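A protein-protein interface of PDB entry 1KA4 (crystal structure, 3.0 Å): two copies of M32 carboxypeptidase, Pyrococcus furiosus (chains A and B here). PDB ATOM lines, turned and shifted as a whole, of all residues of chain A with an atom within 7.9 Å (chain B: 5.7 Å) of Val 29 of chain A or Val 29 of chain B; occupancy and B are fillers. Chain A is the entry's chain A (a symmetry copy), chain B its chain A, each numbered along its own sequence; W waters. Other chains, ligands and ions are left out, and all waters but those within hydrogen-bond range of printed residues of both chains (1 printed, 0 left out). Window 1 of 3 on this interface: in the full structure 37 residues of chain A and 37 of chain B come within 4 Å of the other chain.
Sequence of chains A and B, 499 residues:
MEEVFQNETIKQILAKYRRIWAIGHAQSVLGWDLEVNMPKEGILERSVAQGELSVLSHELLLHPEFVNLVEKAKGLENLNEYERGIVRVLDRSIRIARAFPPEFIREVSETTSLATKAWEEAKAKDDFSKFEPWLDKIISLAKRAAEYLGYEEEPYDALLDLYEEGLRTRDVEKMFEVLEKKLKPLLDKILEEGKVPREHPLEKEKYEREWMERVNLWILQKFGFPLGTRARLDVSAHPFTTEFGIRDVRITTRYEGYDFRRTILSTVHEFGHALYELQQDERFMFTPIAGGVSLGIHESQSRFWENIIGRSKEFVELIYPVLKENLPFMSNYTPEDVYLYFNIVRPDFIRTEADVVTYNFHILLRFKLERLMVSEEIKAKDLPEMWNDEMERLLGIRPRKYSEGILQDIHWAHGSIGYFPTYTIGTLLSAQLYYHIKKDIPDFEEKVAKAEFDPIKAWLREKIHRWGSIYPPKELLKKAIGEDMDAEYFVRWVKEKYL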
ATOM      1  N   ALA A  22       6.411  -7.429   0.527  1.00  0.00           N
ATOM      2  CA  ALA A  22       6.184  -7.575   1.957  1.00  0.00           C
ATOM      3  C   ALA A  22       6.233  -9.044   2.399  1.00  0.00           C
ATOM      4  O   ALA A  22       6.870  -9.382   3.398  1.00  0.00           O
ATOM      5  CB  ALA A  22       4.864  -6.966   2.312  1.00  0.00           C
ATOM      6  N   ILE A  23       5.548  -9.916   1.667  1.00  0.00           N
ATOM      7  CA  ILE A  23       5.578 -11.340   1.993  1.00  0.00           C
ATOM      8  C   ILE A  23       7.047 -11.810   1.954  1.00  0.00           C
ATOM      9  O   ILE A  23       7.473 -12.531   2.848  1.00  0.00           O
ATOM     10  CB  ILE A  23       4.716 -12.158   0.985  1.00  0.00           C
ATOM     11  CG1 ILE A  23       3.238 -11.872   1.220  1.00  0.00           C
ATOM     12  CG2 ILE A  23       4.955 -13.652   1.145  1.00  0.00           C
ATOM     13  CD1 ILE A  23       2.323 -12.589   0.232  1.00  0.00           C
ATOM     14  N   GLY A  24       7.804 -11.390   0.931  1.00  0.00           N
ATOM     15  CA  GLY A  24       9.204 -11.763   0.812  1.00  0.00           C
ATOM     16  C   GLY A  24      10.029 -11.266   1.993  1.00  0.00           C
ATOM     17  O   GLY A  24      10.932 -11.949   2.496  1.00  0.00           O
ATOM     18  N   HIS A  25       9.721 -10.062   2.449  1.00  0.00           N
ATOM     19  CA  HIS A  25      10.417  -9.487   3.596  1.00  0.00           C
ATOM     20  C   HIS A  25      10.174 -10.408   4.779  1.00  0.00           C
ATOM     21  O   HIS A  25      11.071 -10.678   5.566  1.00  0.00           O
ATOM     22  CB  HIS A  25       9.845  -8.106   3.897  1.00  0.00           C
ATOM     23  CG  HIS A  25      10.448  -7.445   5.091  1.00  0.00           C
ATOM     24  ND1 HIS A  25      11.705  -6.883   5.082  1.00  0.00           N
ATOM     25  CD2 HIS A  25       9.950  -7.221   6.330  1.00  0.00           C
ATOM     26  CE1 HIS A  25      11.954  -6.335   6.261  1.00  0.00           C
ATOM     27  NE2 HIS A  25      10.904  -6.525   7.036  1.00  0.00           N
ATOM     28  N   ALA A  26       8.948 -10.890   4.898  1.00  0.00           N
ATOM     29  CA  ALA A  26       8.601 -11.776   5.988  1.00  0.00           C
ATOM     30  C   ALA A  26       9.254 -13.140   5.818  1.00  0.00           C
ATOM     31  O   ALA A  26       9.726 -13.729   6.796  1.00  0.00           O
ATOM     32  CB  ALA A  26       7.092 -11.919   6.084  1.00  0.00           C
ATOM     33  N   GLN A  27       9.290 -13.657   4.591  1.00  0.00           N
ATOM     34  CA  GLN A  27       9.924 -14.948   4.339  1.00  0.00           C
ATOM     35  C   GLN A  27      11.388 -14.888   4.759  1.00  0.00           C
ATOM     36  O   GLN A  27      11.921 -15.846   5.307  1.00  0.00           O
ATOM     37  CB  GLN A  27       9.844 -15.336   2.864  1.00  0.00           C
ATOM     38  CG  GLN A  27       8.497 -15.810   2.358  1.00  0.00           C
ATOM     39  CD  GLN A  27       8.099 -17.182   2.889  1.00  0.00           C
ATOM     40  OE1 GLN A  27       7.279 -17.879   2.274  1.00  0.00           O
ATOM     41  NE2 GLN A  27       8.659 -17.574   4.037  1.00  0.00           N
ATOM     42  N   SER A  28      12.037 -13.757   4.510  1.00  0.00           N
ATOM     43  CA  SER A  28      13.437 -13.604   4.867  1.00  0.00           C
ATOM     44  C   SER A  28      13.635 -13.668   6.362  1.00  0.00           C
ATOM     45  O   SER A  28      14.488 -14.405   6.872  1.00  0.00           O
ATOM     46  CB  SER A  28      13.978 -12.285   4.347  1.00  0.00           C
ATOM     47  OG  SER A  28      14.033 -12.298   2.935  1.00  0.00           O
ATOM     48  N   VAL A  29      12.849 -12.891   7.078  1.00  0.00           N
ATOM     49  CA  VAL A  29      12.962 -12.887   8.511  1.00  0.00           C
ATOM     50  C   VAL A  29      12.703 -14.273   9.085  1.00  0.00           C
ATOM     51  O   VAL A  29      13.388 -14.707  10.009  1.00  0.00           O
ATOM     52  CB  VAL A  29      11.980 -11.927   9.119  1.00  0.00           C
ATOM     53  CG1 VAL A  29      12.081 -11.990  10.633  1.00  0.00           C
ATOM     54  CG2 VAL A  29      12.258 -10.539   8.611  1.00  0.00           C
ATOM     55  N   LEU A  30      11.695 -14.947   8.546  1.00  0.00           N
ATOM     56  CA  LEU A  30      11.333 -16.285   8.990  1.00  0.00           C
ATOM     57  C   LEU A  30      12.486 -17.246   8.787  1.00  0.00           C
ATOM     58  O   LEU A  30      12.827 -18.004   9.695  1.00  0.00           O
ATOM     59  CB  LEU A  30      10.131 -16.785   8.194  1.00  0.00           C
ATOM     60  CG  LEU A  30       8.732 -16.680   8.791  1.00  0.00           C
ATOM     61  CD1 LEU A  30       8.654 -15.554   9.784  1.00  0.00           C
ATOM     62  CD2 LEU A  30       7.732 -16.504   7.662  1.00  0.00           C
ATOM     63  N   GLY A  31      13.073 -17.210   7.591  1.00  0.00           N
ATOM     64  CA  GLY A  31      14.181 -18.082   7.270  1.00  0.00           C
ATOM     65  C   GLY A  31      15.365 -17.824   8.181  1.00  0.00           C
ATOM     66  O   GLY A  31      15.941 -18.736   8.765  1.00  0.00           O
ATOM     67  N   TRP A  32      15.719 -16.554   8.313  1.00  0.00           N
ATOM     68  CA  TRP A  32      16.844 -16.168   9.146  1.00  0.00           C
ATOM     69  C   TRP A  32      16.651 -16.617  10.601  1.00  0.00           C
ATOM     70  O   TRP A  32      17.519 -17.228  11.207  1.00  0.00           O
ATOM     71  CB  TRP A  32      17.025 -14.649   9.072  1.00  0.00           C
ATOM     72  CG  TRP A  32      18.116 -14.125   9.947  1.00  0.00           C
ATOM     73  CD1 TRP A  32      19.446 -14.115   9.677  1.00  0.00           C
ATOM     74  CD2 TRP A  32      17.967 -13.550  11.247  1.00  0.00           C
ATOM     75  NE1 TRP A  32      20.138 -13.572  10.727  1.00  0.00           N
ATOM     76  CE2 TRP A  32      19.249 -13.214  11.704  1.00  0.00           C
ATOM     77  CE3 TRP A  32      16.865 -13.286  12.075  1.00  0.00           C
ATOM     78  CZ2 TRP A  32      19.466 -12.623  12.953  1.00  0.00           C
ATOM     79  CZ3 TRP A  32      17.084 -12.698  13.324  1.00  0.00           C
ATOM     80  CH2 TRP A  32      18.371 -12.376  13.743  1.00  0.00           C
ATOM     81  N   ASP A  33      15.491 -16.309  11.153  1.00  0.00           N
ATOM     82  CA  ASP A  33      15.214 -16.650  12.526  1.00  0.00           C
ATOM     83  C   ASP A  33      15.180 -18.150  12.754  1.00  0.00           C
ATOM     84  O   ASP A  33      15.499 -18.637  13.838  1.00  0.00           O
ATOM     85  CB  ASP A  33      13.896 -16.032  12.935  1.00  0.00           C
ATOM     86  CG  ASP A  33      13.439 -16.529  14.260  1.00  0.00           C
ATOM     87  OD1 ASP A  33      12.708 -17.544  14.289  1.00  0.00           O
ATOM     88  OD2 ASP A  33      13.838 -15.920  15.273  1.00  0.00           O
ATOM     89  N   LEU A  34      14.784 -18.889  11.729  1.00  0.00           N
ATOM     90  CA  LEU A  34      14.750 -20.338  11.857  1.00  0.00           C
ATOM     91  C   LEU A  34      16.182 -20.865  12.073  1.00  0.00           C
ATOM     92  O   LEU A  34      16.421 -21.743  12.905  1.00  0.00           O
ATOM     93  CB  LEU A  34      14.094 -20.957  10.607  1.00  0.00           C
ATOM     94  CG  LEU A  34      14.445 -22.377  10.164  1.00  0.00           C
ATOM     95  CD1 LEU A  34      14.654 -23.287  11.340  1.00  0.00           C
ATOM     96  CD2 LEU A  34      13.334 -22.899   9.304  1.00  0.00           C
ATOM     97  N   GLU A  35      17.136 -20.307  11.342  1.00  0.00           N
ATOM     98  CA  GLU A  35      18.519 -20.728  11.449  1.00  0.00           C
ATOM     99  C   GLU A  35      19.213 -20.160  12.672  1.00  0.00           C
ATOM    100  O   GLU A  35      20.042 -20.825  13.285  1.00  0.00           O
ATOM    101  CB  GLU A  35      19.320 -20.272  10.229  1.00  0.00           C
ATOM    102  CG  GLU A  35      19.001 -20.967   8.942  1.00  0.00           C
ATOM    103  CD  GLU A  35      19.255 -22.440   9.009  1.00  0.00           C
ATOM    104  OE1 GLU A  35      20.340 -22.834   9.504  1.00  0.00           O
ATOM    105  OE2 GLU A  35      18.367 -23.196   8.554  1.00  0.00           O
ATOM    106  N   VAL A  36      18.875 -18.929  13.025  1.00  0.00           N
ATOM    107  CA  VAL A  36      19.552 -18.271  14.115  1.00  0.00           C
ATOM    108  C   VAL A  36      18.947 -18.255  15.505  1.00  0.00           C
ATOM    109  O   VAL A  36      19.700 -18.353  16.467  1.00  0.00           O
ATOM    110  CB  VAL A  36      19.911 -16.824  13.710  1.00  0.00           C
ATOM    111  CG1 VAL A  36      20.520 -16.067  14.868  1.00  0.00           C
ATOM    112  CG2 VAL A  36      20.886 -16.855  12.561  1.00  0.00           C
ATOM    113  N   ASN A  37      17.630 -18.143  15.651  1.00  0.00           N
ATOM    114  CA  ASN A  37      17.065 -18.081  16.998  1.00  0.00           C
ATOM    115  C   ASN A  37      16.025 -19.113  17.411  1.00  0.00           C
ATOM    116  O   ASN A  37      15.947 -19.483  18.570  1.00  0.00           O
ATOM    117  CB  ASN A  37      16.445 -16.698  17.240  1.00  0.00           C
ATOM    118  CG  ASN A  37      17.382 -15.558  16.914  1.00  0.00           C
ATOM    119  OD1 ASN A  37      18.409 -15.370  17.563  1.00  0.00           O
ATOM    120  ND2 ASN A  37      17.030 -14.786  15.902  1.00  0.00           N
ATOM    121  N   ARG A  46       6.745 -23.119  12.066  1.00  0.00           N
ATOM    122  CA  ARG A  46       7.508 -22.226  11.213  1.00  0.00           C
ATOM    123  C   ARG A  46       7.348 -22.707   9.787  1.00  0.00           C
ATOM    124  O   ARG A  46       7.072 -21.913   8.902  1.00  0.00           O
ATOM    125  CB  ARG A  46       8.994 -22.241  11.580  1.00  0.00           C
ATOM    126  CG  ARG A  46       9.884 -21.409  10.658  1.00  0.00           C
ATOM    127  CD  ARG A  46       9.343 -20.005  10.484  1.00  0.00           C
ATOM    128  NE  ARG A  46       9.167 -19.376  11.783  1.00  0.00           N
ATOM    129  CZ  ARG A  46      10.143 -18.803  12.470  1.00  0.00           C
ATOM    130  NH1 ARG A  46      11.362 -18.768  11.983  1.00  0.00           N
ATOM    131  NH2 ARG A  46       9.907 -18.285  13.660  1.00  0.00           N
ATOM    132  N   ALA A  49       3.889 -22.002   8.229  1.00  0.00           N
ATOM    133  CA  ALA A  49       3.774 -20.573   7.954  1.00  0.00           C
ATOM    134  C   ALA A  49       4.501 -20.242   6.667  1.00  0.00           C
ATOM    135  O   ALA A  49       3.965 -19.532   5.801  1.00  0.00           O
ATOM    136  CB  ALA A  49       4.352 -19.769   9.085  1.00  0.00           C
ATOM    137  N   GLN A  50       5.717 -20.768   6.542  1.00  0.00           N
ATOM    138  CA  GLN A  50       6.537 -20.557   5.360  1.00  0.00           C
ATOM    139  C   GLN A  50       5.843 -21.051   4.094  1.00  0.00           C
ATOM    140  O   GLN A  50       5.904 -20.400   3.047  1.00  0.00           O
ATOM    141  CB  GLN A  50       7.867 -21.276   5.514  1.00  0.00           C
ATOM    142  CG  GLN A  50       8.750 -20.654   6.534  1.00  0.00           C
ATOM    143  CD  GLN A  50      10.068 -21.366   6.650  1.00  0.00           C
ATOM    144  OE1 GLN A  50      10.116 -22.571   6.899  1.00  0.00           O
ATOM    145  NE2 GLN A  50      11.157 -20.622   6.482  1.00  0.00           N
ATOM    146  N   THR A 242      21.352 -12.586   4.283  1.00  0.00           N
ATOM    147  CA  THR A 242      19.949 -12.344   3.989  1.00  0.00           C
ATOM    148  C   THR A 242      19.722 -10.869   3.840  1.00  0.00           C
ATOM    149  O   THR A 242      20.408 -10.059   4.447  1.00  0.00           O
ATOM    150  CB  THR A 242      19.031 -12.805   5.103  1.00  0.00           C
ATOM    151  OG1 THR A 242      19.801 -13.500   6.083  1.00  0.00           O
ATOM    152  CG2 THR A 242      17.967 -13.737   4.556  1.00  0.00           C
ATOM    153  N   GLU A 243      18.756 -10.511   3.019  1.00  0.00           N
ATOM    154  CA  GLU A 243      18.437  -9.112   2.837  1.00  0.00           C
ATOM    155  C   GLU A 243      17.001  -8.913   3.267  1.00  0.00           C
ATOM    156  O   GLU A 243      16.076  -9.351   2.589  1.00  0.00           O
ATOM    157  CB  GLU A 243      18.575  -8.699   1.378  1.00  0.00           C
ATOM    158  CG  GLU A 243      19.771  -9.326   0.682  1.00  0.00           C
ATOM    159  CD  GLU A 243      19.485 -10.718   0.105  1.00  0.00           C
ATOM    160  OE1 GLU A 243      18.433 -10.876  -0.556  1.00  0.00           O
ATOM    161  OE2 GLU A 243      20.315 -11.640   0.298  1.00  0.00           O
ATOM    162  N   PHE A 244      16.820  -8.287   4.421  1.00  0.00           N
ATOM    163  CA  PHE A 244      15.498  -7.979   4.906  1.00  0.00           C
ATOM    164  C   PHE A 244      15.165  -6.679   4.181  1.00  0.00           C
ATOM    165  O   PHE A 244      14.007  -6.371   3.910  1.00  0.00           O
ATOM    166  CB  PHE A 244      15.515  -7.750   6.414  1.00  0.00           C
ATOM    167  CG  PHE A 244      15.705  -9.007   7.228  1.00  0.00           C
ATOM    168  CD1 PHE A 244      15.606  -8.959   8.620  1.00  0.00           C
ATOM    169  CD2 PHE A 244      15.933 -10.250   6.612  1.00  0.00           C
ATOM    170  CE1 PHE A 244      15.721 -10.110   9.375  1.00  0.00           C
ATOM    171  CE2 PHE A 244      16.050 -11.417   7.368  1.00  0.00           C
ATOM    172  CZ  PHE A 244      15.942 -11.344   8.749  1.00  0.00           C
ATOM    173  N   GLY A 245      16.208  -5.924   3.854  1.00  0.00           N
ATOM    174  CA  GLY A 245      16.043  -4.664   3.154  1.00  0.00           C
ATOM    175  C   GLY A 245      17.376  -4.029   2.802  1.00  0.00           C
ATOM    176  O   GLY A 245      18.445  -4.550   3.131  1.00  0.00           O
ATOM    177  N   ASP A 248      18.862  -3.219   5.977  1.00  0.00           N
ATOM    178  CA  ASP A 248      18.876  -4.310   6.944  1.00  0.00           C
ATOM    179  C   ASP A 248      19.377  -5.553   6.232  1.00  0.00           C
ATOM    180  O   ASP A 248      18.602  -6.246   5.578  1.00  0.00           O
ATOM    181  CB  ASP A 248      17.464  -4.549   7.486  1.00  0.00           C
ATOM    182  CG  ASP A 248      17.445  -5.460   8.714  1.00  0.00           C
ATOM    183  OD1 ASP A 248      18.472  -6.082   9.017  1.00  0.00           O
ATOM    184  OD2 ASP A 248      16.392  -5.565   9.385  1.00  0.00           O
ATOM    185  N   ARG A 250      21.873  -9.078   6.875  1.00  0.00           N
ATOM    186  CA  ARG A 250      22.532  -9.804   7.950  1.00  0.00           C
ATOM    187  C   ARG A 250      23.326 -10.982   7.468  1.00  0.00           C
ATOM    188  O   ARG A 250      22.949 -11.635   6.500  1.00  0.00           O
ATOM    189  CB  ARG A 250      21.483 -10.271   8.956  1.00  0.00           C
ATOM    190  CG  ARG A 250      20.496  -9.166   9.301  1.00  0.00           C
ATOM    191  CD  ARG A 250      19.456  -9.589  10.312  1.00  0.00           C
ATOM    192  NE  ARG A 250      18.489  -8.514  10.521  1.00  0.00           N
ATOM    193  CZ  ARG A 250      17.508  -8.555  11.417  1.00  0.00           C
ATOM    194  NH1 ARG A 250      17.352  -9.621  12.197  1.00  0.00           N
ATOM    195  NH2 ARG A 250      16.692  -7.520  11.544  1.00  0.00           N
ATOM    196  N   GLY B  24      -0.192 -13.736  10.443  1.00  0.00           N
ATOM    197  CA  GLY B  24      -0.055 -13.388  11.848  1.00  0.00           C
ATOM    198  C   GLY B  24       1.244 -13.918  12.444  1.00  0.00           C
ATOM    199  O   GLY B  24       1.910 -13.260  13.254  1.00  0.00           O
ATOM    200  N   HIS B  25       1.616 -15.122  12.042  1.00  0.00           N
ATOM    201  CA  HIS B  25       2.856 -15.728  12.515  1.00  0.00           C
ATOM    202  C   HIS B  25       3.995 -14.822  12.081  1.00  0.00           C
ATOM    203  O   HIS B  25       4.933 -14.580  12.830  1.00  0.00           O
ATOM    204  CB  HIS B  25       3.026 -17.103  11.878  1.00  0.00           C
ATOM    205  CG  HIS B  25       4.296 -17.794  12.250  1.00  0.00           C
ATOM    206  ND1 HIS B  25       4.498 -18.378  13.479  1.00  0.00           N
ATOM    207  CD2 HIS B  25       5.423 -18.027  11.537  1.00  0.00           C
ATOM    208  CE1 HIS B  25       5.692 -18.949  13.508  1.00  0.00           C
ATOM    209  NE2 HIS B  25       6.272 -18.752  12.341  1.00  0.00           N
ATOM    210  N   ALA B  26       3.905 -14.319  10.861  1.00  0.00           N
ATOM    211  CA  ALA B  26       4.933 -13.443  10.341  1.00  0.00           C
ATOM    212  C   ALA B  26       4.906 -12.090  11.035  1.00  0.00           C
ATOM    213  O   ALA B  26       5.962 -11.524  11.336  1.00  0.00           O
ATOM    214  CB  ALA B  26       4.764 -13.274   8.841  1.00  0.00           C
ATOM    215  N   GLN B  27       3.714 -11.555  11.295  1.00  0.00           N
ATOM    216  CA  GLN B  27       3.602 -10.271  11.984  1.00  0.00           C
ATOM    217  C   GLN B  27       4.273 -10.365  13.350  1.00  0.00           C
ATOM    218  O   GLN B  27       4.924  -9.426  13.792  1.00  0.00           O
ATOM    219  CB  GLN B  27       2.143  -9.859  12.172  1.00  0.00           C
ATOM    220  CG  GLN B  27       1.417  -9.352  10.942  1.00  0.00           C
ATOM    221  CD  GLN B  27       1.895  -7.981  10.478  1.00  0.00           C
ATOM    222  OE1 GLN B  27       1.158  -7.260   9.790  1.00  0.00           O
ATOM    223  NE2 GLN B  27       3.131  -7.618  10.832  1.00  0.00           N
ATOM    224  N   SER B  28       4.121 -11.504  14.014  1.00  0.00           N
ATOM    225  CA  SER B  28       4.717 -11.688  15.327  1.00  0.00           C
ATOM    226  C   SER B  28       6.224 -11.651  15.259  1.00  0.00           C
ATOM    227  O   SER B  28       6.890 -10.938  16.019  1.00  0.00           O
ATOM    228  CB  SER B  28       4.276 -13.009  15.930  1.00  0.00           C
ATOM    229  OG  SER B  28       2.895 -12.975  16.234  1.00  0.00           O
ATOM    230  N   VAL B  29       6.775 -12.425  14.347  1.00  0.00           N
ATOM    231  CA  VAL B  29       8.206 -12.453  14.204  1.00  0.00           C
ATOM    232  C   VAL B  29       8.750 -11.071  13.869  1.00  0.00           C
ATOM    233  O   VAL B  29       9.789 -10.665  14.387  1.00  0.00           O
ATOM    234  CB  VAL B  29       8.613 -13.404  13.116  1.00  0.00           C
ATOM    235  CG1 VAL B  29      10.122 -13.367  12.949  1.00  0.00           C
ATOM    236  CG2 VAL B  29       8.136 -14.788  13.458  1.00  0.00           C
ATOM    237  N   LEU B  30       8.055 -10.371  12.983  1.00  0.00           N
ATOM    238  CA  LEU B  30       8.453  -9.033  12.569  1.00  0.00           C
ATOM    239  C   LEU B  30       8.474  -8.091  13.755  1.00  0.00           C
ATOM    240  O   LEU B  30       9.442  -7.353  13.942  1.00  0.00           O
ATOM    241  CB  LEU B  30       7.467  -8.498  11.535  1.00  0.00           C
ATOM    242  CG  LEU B  30       7.805  -8.587  10.051  1.00  0.00           C
ATOM    243  CD1 LEU B  30       8.748  -9.727   9.781  1.00  0.00           C
ATOM    244  CD2 LEU B  30       6.515  -8.727   9.263  1.00  0.00           C
ATOM    245  N   GLY B  31       7.400  -8.119  14.543  1.00  0.00           N
ATOM    246  CA  GLY B  31       7.295  -7.263  15.704  1.00  0.00           C
ATOM    247  C   GLY B  31       8.396  -7.557  16.704  1.00  0.00           C
ATOM    248  O   GLY B  31       9.090  -6.665  17.183  1.00  0.00           O
ATOM    249  N   TRP B  32       8.565  -8.835  17.010  1.00  0.00           N
ATOM    250  CA  TRP B  32       9.576  -9.255  17.963  1.00  0.00           C
ATOM    251  C   TRP B  32      10.982  -8.826  17.524  1.00  0.00           C
ATOM    252  O   TRP B  32      11.743  -8.239  18.281  1.00  0.00           O
ATOM    253  CB  TRP B  32       9.507 -10.776  18.131  1.00  0.00           C
ATOM    254  CG  TRP B  32      10.551 -11.334  19.042  1.00  0.00           C
ATOM    255  CD1 TRP B  32      10.520 -11.364  20.399  1.00  0.00           C
ATOM    256  CD2 TRP B  32      11.793 -11.926  18.657  1.00  0.00           C
ATOM    257  NE1 TRP B  32      11.664 -11.936  20.886  1.00  0.00           N
ATOM    258  CE2 TRP B  32      12.463 -12.293  19.833  1.00  0.00           C
ATOM    259  CE3 TRP B  32      12.409 -12.182  17.422  1.00  0.00           C
ATOM    260  CZ2 TRP B  32      13.720 -12.906  19.816  1.00  0.00           C
ATOM    261  CZ3 TRP B  32      13.666 -12.794  17.408  1.00  0.00           C
ATOM    262  CH2 TRP B  32      14.299 -13.146  18.596  1.00  0.00           C
ATOM    263  N   ASP B  33      11.315  -9.120  16.280  1.00  0.00           N
ATOM    264  CA  ASP B  33      12.624  -8.795  15.770  1.00  0.00           C
ATOM    265  C   ASP B  33      12.870  -7.299  15.720  1.00  0.00           C
ATOM    266  O   ASP B  33      14.002  -6.835  15.850  1.00  0.00           O
ATOM    267  CB  ASP B  33      12.783  -9.395  14.391  1.00  0.00           C
ATOM    268  CG  ASP B  33      14.015  -8.910  13.715  1.00  0.00           C
ATOM    269  OD1 ASP B  33      13.934  -7.883  13.006  1.00  0.00           O
ATOM    270  OD2 ASP B  33      15.071  -9.542  13.919  1.00  0.00           O
ATOM    271  N   LEU B  34      11.806  -6.536  15.522  1.00  0.00           N
ATOM    272  CA  LEU B  34      11.952  -5.089  15.489  1.00  0.00           C
ATOM    273  C   LEU B  34      12.427  -4.593  16.868  1.00  0.00           C
ATOM    274  O   LEU B  34      13.304  -3.732  16.970  1.00  0.00           O
ATOM    275  CB  LEU B  34      10.618  -4.439  15.074  1.00  0.00           C
ATOM    276  CG  LEU B  34      10.270  -3.019  15.520  1.00  0.00           C
ATOM    277  CD1 LEU B  34      11.481  -2.131  15.532  1.00  0.00           C
ATOM    278  CD2 LEU B  34       9.237  -2.463  14.586  1.00  0.00           C
ATOM    279  N   ARG B  46      10.798  -2.164   7.618  1.00  0.00           N
ATOM    280  CA  ARG B  46      10.077  -3.058   8.505  1.00  0.00           C
ATOM    281  C   ARG B  46       8.654  -2.551   8.606  1.00  0.00           C
ATOM    282  O   ARG B  46       7.719  -3.326   8.479  1.00  0.00           O
ATOM    283  CB  ARG B  46      10.700  -3.076   9.903  1.00  0.00           C
ATOM    284  CG  ARG B  46       9.934  -3.910  10.928  1.00  0.00           C
ATOM    285  CD  ARG B  46       9.642  -5.300  10.405  1.00  0.00           C
ATOM    286  NE  ARG B  46      10.878  -5.946   9.993  1.00  0.00           N
ATOM    287  CZ  ARG B  46      11.715  -6.548  10.823  1.00  0.00           C
ATOM    288  NH1 ARG B  46      11.450  -6.598  12.108  1.00  0.00           N
ATOM    289  NH2 ARG B  46      12.834  -7.079  10.372  1.00  0.00           N
ATOM    290  N   PHE B 244       4.776 -17.060  18.652  1.00  0.00           N
ATOM    291  CA  PHE B 244       5.014 -17.350  17.260  1.00  0.00           C
ATOM    292  C   PHE B 244       4.217 -18.633  17.041  1.00  0.00           C
ATOM    293  O   PHE B 244       3.741 -18.915  15.944  1.00  0.00           O
ATOM    294  CB  PHE B 244       6.497 -17.603  17.007  1.00  0.00           C
ATOM    295  CG  PHE B 244       7.354 -16.363  17.070  1.00  0.00           C
ATOM    296  CD1 PHE B 244       8.706 -16.430  16.726  1.00  0.00           C
ATOM    297  CD2 PHE B 244       6.812 -15.115  17.423  1.00  0.00           C
ATOM    298  CE1 PHE B 244       9.491 -15.294  16.724  1.00  0.00           C
ATOM    299  CE2 PHE B 244       7.598 -13.962  17.422  1.00  0.00           C
ATOM    300  CZ  PHE B 244       8.937 -14.055  17.072  1.00  0.00           C
HETATM  301  O   HOH W   1      14.068  -4.443   8.627  1.00  0.00           O
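Val 29 of chain B touches just these residues of chain A: Val 29 (3.3 Å), Leu 30 (3.8 Å) and Arg 46 (3.9 Å). Printed residues of chain A within 4 Å of Phe 244 of chain B: Arg 46 (3.8 Å). Printed residues of chain B within 4 Å of Ala 49 of chain A: His 25 (3.2 Å). Ala 22 of chain A touches none of the printed residues of chain B. Gln 50 of chain A touches none of the printed residues of chain B. The nearest residue of chain B that does not touch Val 29 of chain A is Asp 33 of chain B (4.6 Å).
A ring nitrogen (NE2) of His 25 of chain B is in hydrogen-bond range of the guanidinium group (NE) of Arg 46 of chain A (3.0 Å). The side-chain carboxylate (OD2) of Asp 33 of chain B lies within salt-bridge range of the guanidinium group (NH1) of Arg 250 of chain A (2.9 Å). A ring nitrogen (NE2) of His 25 of chain A sits at hydrogen-bond distance from the guanidinium group of Arg 46 of chain B, 3.0 Å away. OD2 of Asp 248 of chain A is in salt-bridge range of NH2 of Arg 46 of chain B (3.99 Å).
Of the 25 printed residues of chain A, 11 touch a printed residue of chain B. Printed residues of chain A that touch a printed residue of chain B: His 25, Ala 26, Val 29, Leu 30, Trp 32, Asp 33, Arg 46, Ala 49, Phe 244, Asp 248 and Arg 250. Along chain B the printed residues that touch a printed residue of chain A span positions 25 to 244. Among the printed residues, 15 pairs touch across the chains.
A ring nitrogen (ND1) of His 25 of chain B sits at hydrogen-bond distance from the backbone carbonyl oxygen (O) of Phe 244 of chain B, 2.6 Å away. The side-chain carboxylate of Asp 33 of chain B is in salt-bridge range of the guanidinium group of Arg 46 of chain B, 2.9 Å away. The backbone carbonyl oxygen (O) of Arg 250 of chain A is in hydrogen-bond range of the backbone NH (N) of Thr 242 of chain A (2.9 Å).
His 25 of chain A touches Arg 46 of chain B, and with the chains exchanged Arg 46 of chain A touches His 25 of chain B. Val 29 of chain A touches its own counterpart, Val 29 of chain B. Arg 46 of chain A touches Phe 244 of chain B, and with the chains exchanged Phe 244 of chain A touches Arg 46 of chain B.
Ala 26 of chain A touches Ala 26 of chain B (CB to CB, 3.9 Å). Val 29 of chain A touches Leu 30 of chain B. Val 29 of chain A touches Arg 46 of chain B. Leu 30 of chain A touches Val 29 of chain B (CD1 to CG2, 3.8 Å). Trp 32 of chain A touches Asp 33 of chain B. Asp 33 of chain A touches Trp 32 of chain B (OD2 to CZ3, 3.8 Å). Val 29 of chain B touches Arg 46 of chain A.
Water W1 bridges the side-chain carboxylate (OD2) of Asp 248 of chain A (2.7 Å) and the guanidinium group (NH2) of Arg 46 of chain B (3.4 Å).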
